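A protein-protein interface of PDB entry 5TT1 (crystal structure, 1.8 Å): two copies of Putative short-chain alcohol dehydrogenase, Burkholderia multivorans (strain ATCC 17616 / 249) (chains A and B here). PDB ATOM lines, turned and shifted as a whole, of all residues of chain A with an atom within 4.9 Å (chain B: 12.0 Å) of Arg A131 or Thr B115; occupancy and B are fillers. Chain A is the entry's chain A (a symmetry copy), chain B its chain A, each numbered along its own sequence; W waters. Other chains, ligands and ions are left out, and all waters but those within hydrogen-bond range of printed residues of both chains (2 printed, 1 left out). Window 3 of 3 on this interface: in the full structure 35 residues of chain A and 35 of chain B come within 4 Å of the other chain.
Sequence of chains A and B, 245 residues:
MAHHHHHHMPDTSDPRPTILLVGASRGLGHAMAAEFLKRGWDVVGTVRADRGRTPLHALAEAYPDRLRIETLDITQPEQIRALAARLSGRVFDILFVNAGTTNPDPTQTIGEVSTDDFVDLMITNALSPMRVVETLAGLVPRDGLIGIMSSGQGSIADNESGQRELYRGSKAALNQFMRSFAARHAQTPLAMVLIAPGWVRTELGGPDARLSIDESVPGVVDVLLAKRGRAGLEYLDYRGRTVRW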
ATOM      1  N   PRO A  77      -6.587  22.026   7.882  1.00  0.00           N
ATOM      2  CA  PRO A  77      -6.861  23.156   6.981  1.00  0.00           C
ATOM      3  C   PRO A  77      -8.193  23.814   7.243  1.00  0.00           C
ATOM      4  O   PRO A  77      -8.333  25.015   6.989  1.00  0.00           O
ATOM      5  CB  PRO A  77      -6.828  22.521   5.580  1.00  0.00           C
ATOM      6  CG  PRO A  77      -6.264  21.152   5.755  1.00  0.00           C
ATOM      7  CD  PRO A  77      -6.517  20.739   7.166  1.00  0.00           C
ATOM      8  N   ILE A  80      -7.684  26.714   9.629  1.00  0.00           N
ATOM      9  CA  ILE A  80      -7.108  27.896   8.993  1.00  0.00           C
ATOM     10  C   ILE A  80      -8.183  28.653   8.217  1.00  0.00           C
ATOM     11  O   ILE A  80      -8.239  29.887   8.243  1.00  0.00           O
ATOM     12  CB  ILE A  80      -5.956  27.505   8.054  1.00  0.00           C
ATOM     13  CG1 ILE A  80      -4.971  26.526   8.705  1.00  0.00           C
ATOM     14  CG2 ILE A  80      -5.230  28.749   7.573  1.00  0.00           C
ATOM     15  CD1 ILE A  80      -3.999  26.025   7.714  1.00  0.00           C
ATOM     16  N   ILE A 123       4.965  17.536   6.836  1.00  0.00           N
ATOM     17  CA  ILE A 123       3.657  18.175   6.966  1.00  0.00           C
ATOM     18  C   ILE A 123       3.739  19.393   7.883  1.00  0.00           C
ATOM     19  O   ILE A 123       3.244  20.477   7.550  1.00  0.00           O
ATOM     20  CB  ILE A 123       2.607  17.163   7.463  1.00  0.00           C
ATOM     21  CG1 ILE A 123       2.192  16.254   6.314  1.00  0.00           C
ATOM     22  CG2 ILE A 123       1.371  17.897   8.014  1.00  0.00           C
ATOM     23  CD1 ILE A 123       1.344  15.043   6.732  1.00  0.00           C
ATOM     24  N   LEU A 127       4.292  21.690   4.404  1.00  0.00           N
ATOM     25  CA  LEU A 127       2.940  21.794   3.856  1.00  0.00           C
ATOM     26  C   LEU A 127       2.095  22.773   4.664  1.00  0.00           C
ATOM     27  O   LEU A 127       1.470  23.685   4.101  1.00  0.00           O
ATOM     28  CB  LEU A 127       2.275  20.415   3.809  1.00  0.00           C
ATOM     29  CG  LEU A 127       0.835  20.454   3.313  1.00  0.00           C
ATOM     30  CD1 LEU A 127       0.751  20.964   1.851  1.00  0.00           C
ATOM     31  CD2 LEU A 127       0.153  19.107   3.494  1.00  0.00           C
ATOM     32  N   SER A 128       2.085  22.623   5.984  1.00  0.00           N
ATOM     33  CA  SER A 128       1.188  23.417   6.826  1.00  0.00           C
ATOM     34  C   SER A 128       1.528  24.908   6.850  1.00  0.00           C
ATOM     35  O   SER A 128       0.609  25.727   6.746  1.00  0.00           O
ATOM     36  CB  SER A 128       1.183  22.858   8.257  1.00  0.00           C
ATOM     37  OG  SER A 128       0.701  21.528   8.278  1.00  0.00           O
ATOM     38  N   PRO A 129       2.795  25.331   6.979  1.00  0.00           N
ATOM     39  CA  PRO A 129       3.037  26.781   6.873  1.00  0.00           C
ATOM     40  C   PRO A 129       2.646  27.335   5.518  1.00  0.00           C
ATOM     41  O   PRO A 129       2.143  28.455   5.445  1.00  0.00           O
ATOM     42  CB  PRO A 129       4.542  26.952   7.151  1.00  0.00           C
ATOM     43  CG  PRO A 129       5.116  25.588   7.218  1.00  0.00           C
ATOM     44  CD  PRO A 129       4.015  24.579   7.346  1.00  0.00           C
ATOM     45  N   MET A 130       2.849  26.581   4.431  1.00  0.00           N
ATOM     46  CA  MET A 130       2.410  27.094   3.143  1.00  0.00           C
ATOM     47  C   MET A 130       0.893  27.184   3.069  1.00  0.00           C
ATOM     48  O   MET A 130       0.368  28.089   2.423  1.00  0.00           O
ATOM     49  CB  MET A 130       2.966  26.239   2.003  1.00  0.00           C
ATOM     50  CG  MET A 130       4.457  26.479   1.772  1.00  0.00           C
ATOM     51  SD  MET A 130       4.851  28.256   1.555  1.00  0.00           S
ATOM     52  CE  MET A 130       3.760  28.743   0.219  1.00  0.00           C
ATOM     53  N   ARG A 131       0.168  26.257   3.703  1.00  0.00           N
ATOM     54  CA  ARG A 131      -1.288  26.382   3.691  1.00  0.00           C
ATOM     55  C   ARG A 131      -1.730  27.605   4.482  1.00  0.00           C
ATOM     56  O   ARG A 131      -2.709  28.263   4.110  1.00  0.00           O
ATOM     57  CB  ARG A 131      -1.948  25.123   4.250  1.00  0.00           C
ATOM     58  CG  ARG A 131      -1.904  23.930   3.300  1.00  0.00           C
ATOM     59  CD  ARG A 131      -2.362  22.671   3.997  1.00  0.00           C
ATOM     60  NE  ARG A 131      -2.667  21.596   3.048  1.00  0.00           N
ATOM     61  CZ  ARG A 131      -3.083  20.388   3.397  1.00  0.00           C
ATOM     62  NH1 ARG A 131      -3.238  20.091   4.680  1.00  0.00           N
ATOM     63  NH2 ARG A 131      -3.341  19.475   2.464  1.00  0.00           N
ATOM     64  N   VAL A 132      -1.009  27.937   5.558  1.00  0.00           N
ATOM     65  CA  VAL A 132      -1.331  29.153   6.309  1.00  0.00           C
ATOM     66  C   VAL A 132      -1.160  30.376   5.415  1.00  0.00           C
ATOM     67  O   VAL A 132      -2.048  31.232   5.320  1.00  0.00           O
ATOM     68  CB  VAL A 132      -0.465  29.249   7.579  1.00  0.00           C
ATOM     69  CG1 VAL A 132      -0.654  30.601   8.288  1.00  0.00           C
ATOM     70  CG2 VAL A 132      -0.763  28.109   8.531  1.00  0.00           C
ATOM     71  N   VAL A 133      -0.015  30.462   4.733  1.00  0.00           N
ATOM     72  CA  VAL A 133       0.260  31.585   3.838  1.00  0.00           C
ATOM     73  C   VAL A 133      -0.835  31.718   2.784  1.00  0.00           C
ATOM     74  O   VAL A 133      -1.427  32.789   2.610  1.00  0.00           O
ATOM     75  CB  VAL A 133       1.642  31.402   3.188  1.00  0.00           C
ATOM     76  CG1 VAL A 133       1.837  32.386   2.043  1.00  0.00           C
ATOM     77  CG2 VAL A 133       2.745  31.532   4.263  1.00  0.00           C
ATOM     78  N   GLU A 134      -1.134  30.621   2.074  1.00  0.00           N
ATOM     79  CA  GLU A 134      -2.088  30.675   0.966  1.00  0.00           C
ATOM     80  C   GLU A 134      -3.497  31.044   1.438  1.00  0.00           C
ATOM     81  O   GLU A 134      -4.227  31.751   0.736  1.00  0.00           O
ATOM     82  CB  GLU A 134      -2.123  29.329   0.229  1.00  0.00           C
ATOM     83  CG  GLU A 134      -0.809  28.881  -0.396  1.00  0.00           C
ATOM     84  CD  GLU A 134      -0.805  29.028  -1.903  1.00  0.00           C
ATOM     85  OE1 GLU A 134      -1.363  30.027  -2.401  1.00  0.00           O
ATOM     86  OE2 GLU A 134      -0.257  28.142  -2.592  1.00  0.00           O
ATOM     87  N   THR A 135      -3.902  30.563   2.616  1.00  0.00           N
ATOM     88  CA  THR A 135      -5.273  30.766   3.088  1.00  0.00           C
ATOM     89  C   THR A 135      -5.460  32.139   3.725  1.00  0.00           C
ATOM     90  O   THR A 135      -6.525  32.753   3.575  1.00  0.00           O
ATOM     91  CB  THR A 135      -5.650  29.662   4.083  1.00  0.00           C
ATOM     92  OG1 THR A 135      -5.564  28.387   3.437  1.00  0.00           O
ATOM     93  CG2 THR A 135      -7.076  29.840   4.633  1.00  0.00           C
ATOM     94  N   LEU A 136      -4.448  32.643   4.435  1.00  0.00           N
ATOM     95  CA  LEU A 136      -4.548  33.924   5.123  1.00  0.00           C
ATOM     96  C   LEU A 136      -3.943  35.070   4.323  1.00  0.00           C
ATOM     97  O   LEU A 136      -3.962  36.206   4.797  1.00  0.00           O
ATOM     98  CB  LEU A 136      -3.872  33.857   6.497  1.00  0.00           C
ATOM     99  CG  LEU A 136      -4.317  32.724   7.430  1.00  0.00           C
ATOM    100  CD1 LEU A 136      -3.624  32.813   8.780  1.00  0.00           C
ATOM    101  CD2 LEU A 136      -5.827  32.716   7.597  1.00  0.00           C
ATOM    102  N   ASN B 103       2.997  14.614  -9.918  1.00  0.00           N
ATOM    103  CA  ASN B 103       1.560  14.598  -9.681  1.00  0.00           C
ATOM    104  C   ASN B 103       0.811  14.647 -11.013  1.00  0.00           C
ATOM    105  O   ASN B 103       1.269  15.287 -11.961  1.00  0.00           O
ATOM    106  CB  ASN B 103       1.142  15.784  -8.818  1.00  0.00           C
ATOM    107  CG  ASN B 103      -0.316  15.724  -8.418  1.00  0.00           C
ATOM    108  OD1 ASN B 103      -1.211  16.148  -9.170  1.00  0.00           O
ATOM    109  ND2 ASN B 103      -0.574  15.164  -7.244  1.00  0.00           N
ATOM    110  N   PRO B 104      -0.339  13.972 -11.115  1.00  0.00           N
ATOM    111  CA  PRO B 104      -1.092  13.999 -12.385  1.00  0.00           C
ATOM    112  C   PRO B 104      -1.522  15.389 -12.818  1.00  0.00           C
ATOM    113  O   PRO B 104      -1.718  15.618 -14.020  1.00  0.00           O
ATOM    114  CB  PRO B 104      -2.312  13.117 -12.091  1.00  0.00           C
ATOM    115  CG  PRO B 104      -1.901  12.267 -10.923  1.00  0.00           C
ATOM    116  CD  PRO B 104      -0.953  13.080 -10.117  1.00  0.00           C
ATOM    117  N   GLN B 108      -1.301  22.288  -9.862  1.00  0.00           N
ATOM    118  CA  GLN B 108      -1.768  22.590  -8.510  1.00  0.00           C
ATOM    119  C   GLN B 108      -0.763  23.457  -7.756  1.00  0.00           C
ATOM    120  O   GLN B 108       0.445  23.188  -7.773  1.00  0.00           O
ATOM    121  CB  GLN B 108      -1.982  21.304  -7.722  1.00  0.00           C
ATOM    122  CG  GLN B 108      -3.165  20.446  -8.113  1.00  0.00           C
ATOM    123  CD  GLN B 108      -3.391  19.344  -7.095  1.00  0.00           C
ATOM    124  OE1 GLN B 108      -2.442  18.664  -6.672  1.00  0.00           O
ATOM    125  NE2 GLN B 108      -4.630  19.193  -6.655  1.00  0.00           N
ATOM    126  N   THR B 109      -1.269  24.479  -7.058  1.00  0.00           N
ATOM    127  CA  THR B 109      -0.435  25.223  -6.122  1.00  0.00           C
ATOM    128  C   THR B 109      -0.243  24.413  -4.844  1.00  0.00           C
ATOM    129  O   THR B 109      -1.036  23.516  -4.533  1.00  0.00           O
ATOM    130  CB  THR B 109      -1.064  26.575  -5.767  1.00  0.00           C
ATOM    131  OG1 THR B 109      -2.256  26.354  -4.998  1.00  0.00           O
ATOM    132  CG2 THR B 109      -1.406  27.382  -7.032  1.00  0.00           C
ATOM    133  N   ILE B 110       0.806  24.754  -4.078  1.00  0.00           N
ATOM    134  CA  ILE B 110       1.037  24.041  -2.817  1.00  0.00           C
ATOM    135  C   ILE B 110      -0.175  24.181  -1.903  1.00  0.00           C
ATOM    136  O   ILE B 110      -0.527  23.246  -1.175  1.00  0.00           O
ATOM    137  CB  ILE B 110       2.336  24.521  -2.124  1.00  0.00           C
ATOM    138  CG1 ILE B 110       2.584  23.737  -0.832  1.00  0.00           C
ATOM    139  CG2 ILE B 110       2.286  25.999  -1.788  1.00  0.00           C
ATOM    140  CD1 ILE B 110       2.706  22.248  -1.070  1.00  0.00           C
ATOM    141  N   GLY B 111      -0.854  25.332  -1.949  1.00  0.00           N
ATOM    142  CA  GLY B 111      -2.048  25.507  -1.145  1.00  0.00           C
ATOM    143  C   GLY B 111      -3.212  24.651  -1.580  1.00  0.00           C
ATOM    144  O   GLY B 111      -4.141  24.440  -0.787  1.00  0.00           O
ATOM    145  N   GLU B 112      -3.183  24.149  -2.816  1.00  0.00           N
ATOM    146  CA  GLU B 112      -4.292  23.376  -3.370  1.00  0.00           C
ATOM    147  C   GLU B 112      -4.141  21.864  -3.181  1.00  0.00           C
ATOM    148  O   GLU B 112      -5.152  21.151  -3.148  1.00  0.00           O
ATOM    149  CB  GLU B 112      -4.431  23.659  -4.865  1.00  0.00           C
ATOM    150  CG  GLU B 112      -5.087  24.967  -5.174  1.00  0.00           C
ATOM    151  CD  GLU B 112      -4.895  25.387  -6.611  1.00  0.00           C
ATOM    152  OE1 GLU B 112      -4.326  24.614  -7.402  1.00  0.00           O
ATOM    153  OE2 GLU B 112      -5.311  26.509  -6.941  1.00  0.00           O
ATOM    154  N   VAL B 113      -2.914  21.353  -3.063  1.00  0.00           N
ATOM    155  CA  VAL B 113      -2.714  19.903  -3.126  1.00  0.00           C
ATOM    156  C   VAL B 113      -3.372  19.221  -1.931  1.00  0.00           C
ATOM    157  O   VAL B 113      -3.506  19.801  -0.850  1.00  0.00           O
ATOM    158  CB  VAL B 113      -1.216  19.561  -3.203  1.00  0.00           C
ATOM    159  CG1 VAL B 113      -0.584  20.262  -4.394  1.00  0.00           C
ATOM    160  CG2 VAL B 113      -0.506  19.923  -1.885  1.00  0.00           C
ATOM    161  N   SER B 114      -3.811  17.980  -2.128  1.00  0.00           N
ATOM    162  CA  SER B 114      -4.312  17.238  -0.982  1.00  0.00           C
ATOM    163  C   SER B 114      -3.151  16.769  -0.107  1.00  0.00           C
ATOM    164  O   SER B 114      -2.007  16.652  -0.556  1.00  0.00           O
ATOM    165  CB  SER B 114      -5.147  16.039  -1.435  1.00  0.00           C
ATOM    166  OG  SER B 114      -4.311  15.074  -2.050  1.00  0.00           O
ATOM    167  N   THR B 115      -3.455  16.468   1.156  1.00  0.00           N
ATOM    168  CA  THR B 115      -2.412  15.906   2.013  1.00  0.00           C
ATOM    169  C   THR B 115      -1.858  14.613   1.420  1.00  0.00           C
ATOM    170  O   THR B 115      -0.649  14.359   1.491  1.00  0.00           O
ATOM    171  CB  THR B 115      -2.954  15.677   3.416  1.00  0.00           C
ATOM    172  OG1 THR B 115      -3.553  16.897   3.882  1.00  0.00           O
ATOM    173  CG2 THR B 115      -1.805  15.270   4.366  1.00  0.00           C
ATOM    174  N   ASP B 116      -2.723  13.811   0.779  1.00  0.00           N
ATOM    175  CA  ASP B 116      -2.278  12.577   0.124  1.00  0.00           C
ATOM    176  C   ASP B 116      -1.330  12.867  -1.042  1.00  0.00           C
ATOM    177  O   ASP B 116      -0.281  12.223  -1.166  1.00  0.00           O
ATOM    178  CB  ASP B 116      -3.482  11.764  -0.353  1.00  0.00           C
ATOM    179  CG  ASP B 116      -4.190  11.041   0.783  1.00  0.00           C
ATOM    180  OD1 ASP B 116      -3.671  11.062   1.918  1.00  0.00           O
ATOM    181  OD2 ASP B 116      -5.270  10.457   0.542  1.00  0.00           O
ATOM    182  N   ASP B 117      -1.702  13.816  -1.916  1.00  0.00           N
ATOM    183  CA  ASP B 117      -0.801  14.305  -2.964  1.00  0.00           C
ATOM    184  C   ASP B 117       0.577  14.610  -2.397  1.00  0.00           C
ATOM    185  O   ASP B 117       1.605  14.197  -2.948  1.00  0.00           O
ATOM    186  CB  ASP B 117      -1.343  15.601  -3.596  1.00  0.00           C
ATOM    187  CG  ASP B 117      -2.589  15.413  -4.447  1.00  0.00           C
ATOM    188  OD1 ASP B 117      -2.843  14.284  -4.922  1.00  0.00           O
ATOM    189  OD2 ASP B 117      -3.301  16.443  -4.656  1.00  0.00           O
ATOM    190  N   PHE B 118       0.608  15.391  -1.317  1.00  0.00           N
ATOM    191  CA  PHE B 118       1.870  15.903  -0.792  1.00  0.00           C
ATOM    192  C   PHE B 118       2.710  14.777  -0.208  1.00  0.00           C
ATOM    193  O   PHE B 118       3.895  14.633  -0.531  1.00  0.00           O
ATOM    194  CB  PHE B 118       1.574  16.964   0.277  1.00  0.00           C
ATOM    195  CG  PHE B 118       2.785  17.389   1.065  1.00  0.00           C
ATOM    196  CD1 PHE B 118       3.602  18.401   0.593  1.00  0.00           C
ATOM    197  CD2 PHE B 118       3.089  16.802   2.294  1.00  0.00           C
ATOM    198  CE1 PHE B 118       4.712  18.824   1.307  1.00  0.00           C
ATOM    199  CE2 PHE B 118       4.225  17.210   3.032  1.00  0.00           C
ATOM    200  CZ  PHE B 118       5.040  18.231   2.526  1.00  0.00           C
ATOM    201  N   VAL B 119       2.095  13.962   0.645  1.00  0.00           N
ATOM    202  CA  VAL B 119       2.799  12.857   1.290  1.00  0.00           C
ATOM    203  C   VAL B 119       3.328  11.876   0.257  1.00  0.00           C
ATOM    204  O   VAL B 119       4.509  11.497   0.290  1.00  0.00           O
ATOM    205  CB  VAL B 119       1.874  12.166   2.302  1.00  0.00           C
ATOM    206  CG1 VAL B 119       2.536  10.875   2.812  1.00  0.00           C
ATOM    207  CG2 VAL B 119       1.580  13.134   3.449  1.00  0.00           C
ATOM    208  N   ASP B 120       2.467  11.455  -0.683  1.00  0.00           N
ATOM    209  CA  ASP B 120       2.876  10.465  -1.686  1.00  0.00           C
ATOM    210  C   ASP B 120       4.095  10.933  -2.464  1.00  0.00           C
ATOM    211  O   ASP B 120       5.077  10.192  -2.602  1.00  0.00           O
ATOM    212  CB  ASP B 120       1.732  10.169  -2.661  1.00  0.00           C
ATOM    213  CG  ASP B 120       0.567   9.445  -2.003  1.00  0.00           C
ATOM    214  OD1 ASP B 120       0.769   8.809  -0.939  1.00  0.00           O
ATOM    215  OD2 ASP B 120      -0.553   9.519  -2.556  1.00  0.00           O
ATOM    216  N   LEU B 121       4.062  12.171  -2.984  1.00  0.00           N
ATOM    217  CA  LEU B 121       5.173  12.623  -3.821  1.00  0.00           C
ATOM    218  C   LEU B 121       6.436  12.907  -3.005  1.00  0.00           C
ATOM    219  O   LEU B 121       7.546  12.738  -3.523  1.00  0.00           O
ATOM    220  CB  LEU B 121       4.785  13.866  -4.636  1.00  0.00           C
ATOM    221  CG  LEU B 121       5.677  14.074  -5.869  1.00  0.00           C
ATOM    222  CD1 LEU B 121       5.334  13.079  -6.986  1.00  0.00           C
ATOM    223  CD2 LEU B 121       5.650  15.494  -6.414  1.00  0.00           C
ATOM    224  N   MET B 122       6.302  13.355  -1.756  1.00  0.00           N
ATOM    225  CA  MET B 122       7.492  13.536  -0.922  1.00  0.00           C
ATOM    226  C   MET B 122       8.147  12.192  -0.620  1.00  0.00           C
ATOM    227  O   MET B 122       9.383  12.083  -0.583  1.00  0.00           O
ATOM    228  CB  MET B 122       7.140  14.254   0.383  1.00  0.00           C
ATOM    229  CG  MET B 122       6.770  15.732   0.217  1.00  0.00           C
ATOM    230  SD  MET B 122       7.971  16.720  -0.698  1.00  0.00           S
ATOM    231  CE  MET B 122       9.447  16.393   0.204  1.00  0.00           C
ATOM    232  N   ILE B 123       7.333  11.155  -0.424  1.00  0.00           N
ATOM    233  CA  ILE B 123       7.874   9.818  -0.191  1.00  0.00           C
ATOM    234  C   ILE B 123       8.529   9.271  -1.457  1.00  0.00           C
ATOM    235  O   ILE B 123       9.657   8.764  -1.424  1.00  0.00           O
ATOM    236  CB  ILE B 123       6.776   8.873   0.332  1.00  0.00           C
ATOM    237  CG1 ILE B 123       6.512   9.163   1.803  1.00  0.00           C
ATOM    238  CG2 ILE B 123       7.205   7.404   0.163  1.00  0.00           C
ATOM    239  CD1 ILE B 123       5.268   8.469   2.378  1.00  0.00           C
ATOM    240  N   THR B 124       7.843   9.354  -2.593  1.00  0.00           N
ATOM    241  CA  THR B 124       8.421   8.752  -3.794  1.00  0.00           C
ATOM    242  C   THR B 124       9.641   9.522  -4.280  1.00  0.00           C
ATOM    243  O   THR B 124      10.584   8.916  -4.793  1.00  0.00           O
ATOM    244  CB  THR B 124       7.391   8.645  -4.930  1.00  0.00           C
ATOM    245  OG1 THR B 124       6.876   9.947  -5.275  1.00  0.00           O
ATOM    246  CG2 THR B 124       6.247   7.709  -4.548  1.00  0.00           C
ATOM    247  N   GLU B 165       4.548  22.996  -8.738  1.00  0.00           N
ATOM    248  CA  GLU B 165       4.983  23.431  -7.413  1.00  0.00           C
ATOM    249  C   GLU B 165       5.320  22.262  -6.502  1.00  0.00           C
ATOM    250  O   GLU B 165       6.325  22.305  -5.779  1.00  0.00           O
ATOM    251  CB  GLU B 165       3.923  24.328  -6.774  1.00  0.00           C
ATOM    252  CG  GLU B 165       3.745  25.620  -7.543  1.00  0.00           C
ATOM    253  CD  GLU B 165       3.137  26.723  -6.707  1.00  0.00           C
ATOM    254  OE1 GLU B 165       2.833  26.479  -5.515  1.00  0.00           O
ATOM    255  OE2 GLU B 165       2.970  27.837  -7.246  1.00  0.00           O
ATOM    256  N   LEU B 166       4.488  21.221  -6.493  1.00  0.00           N
ATOM    257  CA  LEU B 166       4.757  20.113  -5.584  1.00  0.00           C
ATOM    258  C   LEU B 166       6.031  19.386  -5.991  1.00  0.00           C
ATOM    259  O   LEU B 166       6.872  19.048  -5.136  1.00  0.00           O
ATOM    260  CB  LEU B 166       3.560  19.162  -5.550  1.00  0.00           C
ATOM    261  CG  LEU B 166       3.714  17.975  -4.594  1.00  0.00           C
ATOM    262  CD1 LEU B 166       3.974  18.428  -3.159  1.00  0.00           C
ATOM    263  CD2 LEU B 166       2.502  17.059  -4.673  1.00  0.00           C
ATOM    264  N   SER B 170       9.619  18.675  -3.885  1.00  0.00           N
ATOM    265  CA  SER B 170      10.120  17.321  -3.654  1.00  0.00           C
ATOM    266  C   SER B 170      11.579  17.207  -4.080  1.00  0.00           C
ATOM    267  O   SER B 170      12.390  16.559  -3.407  1.00  0.00           O
ATOM    268  CB  SER B 170       9.243  16.304  -4.395  1.00  0.00           C
ATOM    269  OG  SER B 170       9.465  16.286  -5.805  1.00  0.00           O
HETATM  270  O   HOH W   1      -3.286  28.456  -4.192  1.00  0.00           O
HETATM  271  O   HOH W   2      -4.330  17.579   6.131  1.00  0.00           O
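The backbone NH (N) of Gly B111 lies within hydrogen-bond range of the side-chain carboxylate (OE2) of Glu A134, 2.9 Å away.
NH2 of Arg A131 lies within hydrogen-bond range of O of Val B113 (3.3 Å).
OG1 of Thr B115 lies within hydrogen-bond range of NH2 of Arg A131 (2.9 Å).
The side-chain carboxylate (OE1) of Glu B112 sits at hydrogen-bond distance from the backbone NH (N) of Thr B109, at 3.1 Å.
The backbone NH (N) of Ile B110 lies within hydrogen-bond range of the side-chain carboxylate (OE1) of Glu B165 (3.0 Å).
The side-chain hydroxyl (OG) of Ser B114 lies close to the backbone NH (N) of Asp B116, at 3.5 Å.
N of Asp B117 lies within hydrogen-bond range of OG of Ser B114 (2.9 Å).
The backbone carbonyl oxygen (O) of Ile A123 lies within hydrogen-bond range of the side-chain hydroxyl (OG) of Ser A128 (2.8 Å).
The side-chain hydroxyl of Thr A135 lies within hydrogen-bond range of the backbone carbonyl oxygen of Arg A131 (2.9 Å).
Ile A123 touches Thr B115.
Ile A123 touches Phe B118 (N to CE2, 3.9 Å).
Ile A123 touches Val B119.
Leu A127 touches Ile B110.
Phe B118 touches Leu A127 (CZ to CB, 3.7 Å).
Met A130 touches Ile B110 (CE to CG2, 3.7 Å).
Ser B114 touches Arg A131.
Glu A134 touches Thr B109 (OE2 to OG1, 3.6 Å).
OE2 of Glu A134 touches CG2 of Ile B110, 3.4 Å away.
Arg A131 touches three residues of chain B.
No residue of chain B comes within 4 Å of Ile A80.
Ser A128 touches none of the printed residues of chain B.
Of chain B, only Ile B110 comes within 4 Å of Met A130.
No residue of chain B comes within 4 Å of Val A132.
No residue of chain B comes within 4 Å of Val A133.
No residue of chain B comes within 4 Å of Thr A135.
Of the printed residues of chain A, Gly B111 touches Glu A134 (2.9 Å).
Of the printed residues of chain A, Val B119 touches Ile A123 (3.8 Å).
Of the printed residues of chain A, Phe B118 touches Ile A123 (3.9 Å) and Leu A127 (3.7 Å).
Of the printed residues of chain A, Val B113 touches Arg A131.
Leu A136 touches none of the printed residues of chain B.
The nearest residue of chain A that does not touch Thr B115 is Leu A127 (4.3 Å).
Of the 13 printed residues of chain A, 5 touch a printed residue of chain B.
Printed residues of chain A that touch a printed residue of chain B: Ile A123, Leu A127, Met A130, Arg A131 and Glu A134.
Hydrophobic or aromatic side chains of chain A that line the printed part of chain B: Ile A123, Leu A127 and Met A130.
Of the 22 printed residues of chain B, 8 touch a printed residue of chain A.
Hydrophobic or aromatic side chains of chain B within 4 Å of the printed part of chain A: Ile B110, Phe B118 and Val B119.
Position printed for both chains: 123.
Of the 12 pairs that touch across the chains among the printed residues, none has its exchanged pair printed and touching as well.
Water W1 lies within hydrogen-bond range of OG1 of Thr B109 (2.5 Å) and OE1 of Glu A134 (3.1 Å).
Water W2 bridges OG1 of Thr B115 (2.5 Å) and NH1 of Arg A131 (3.1 Å).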
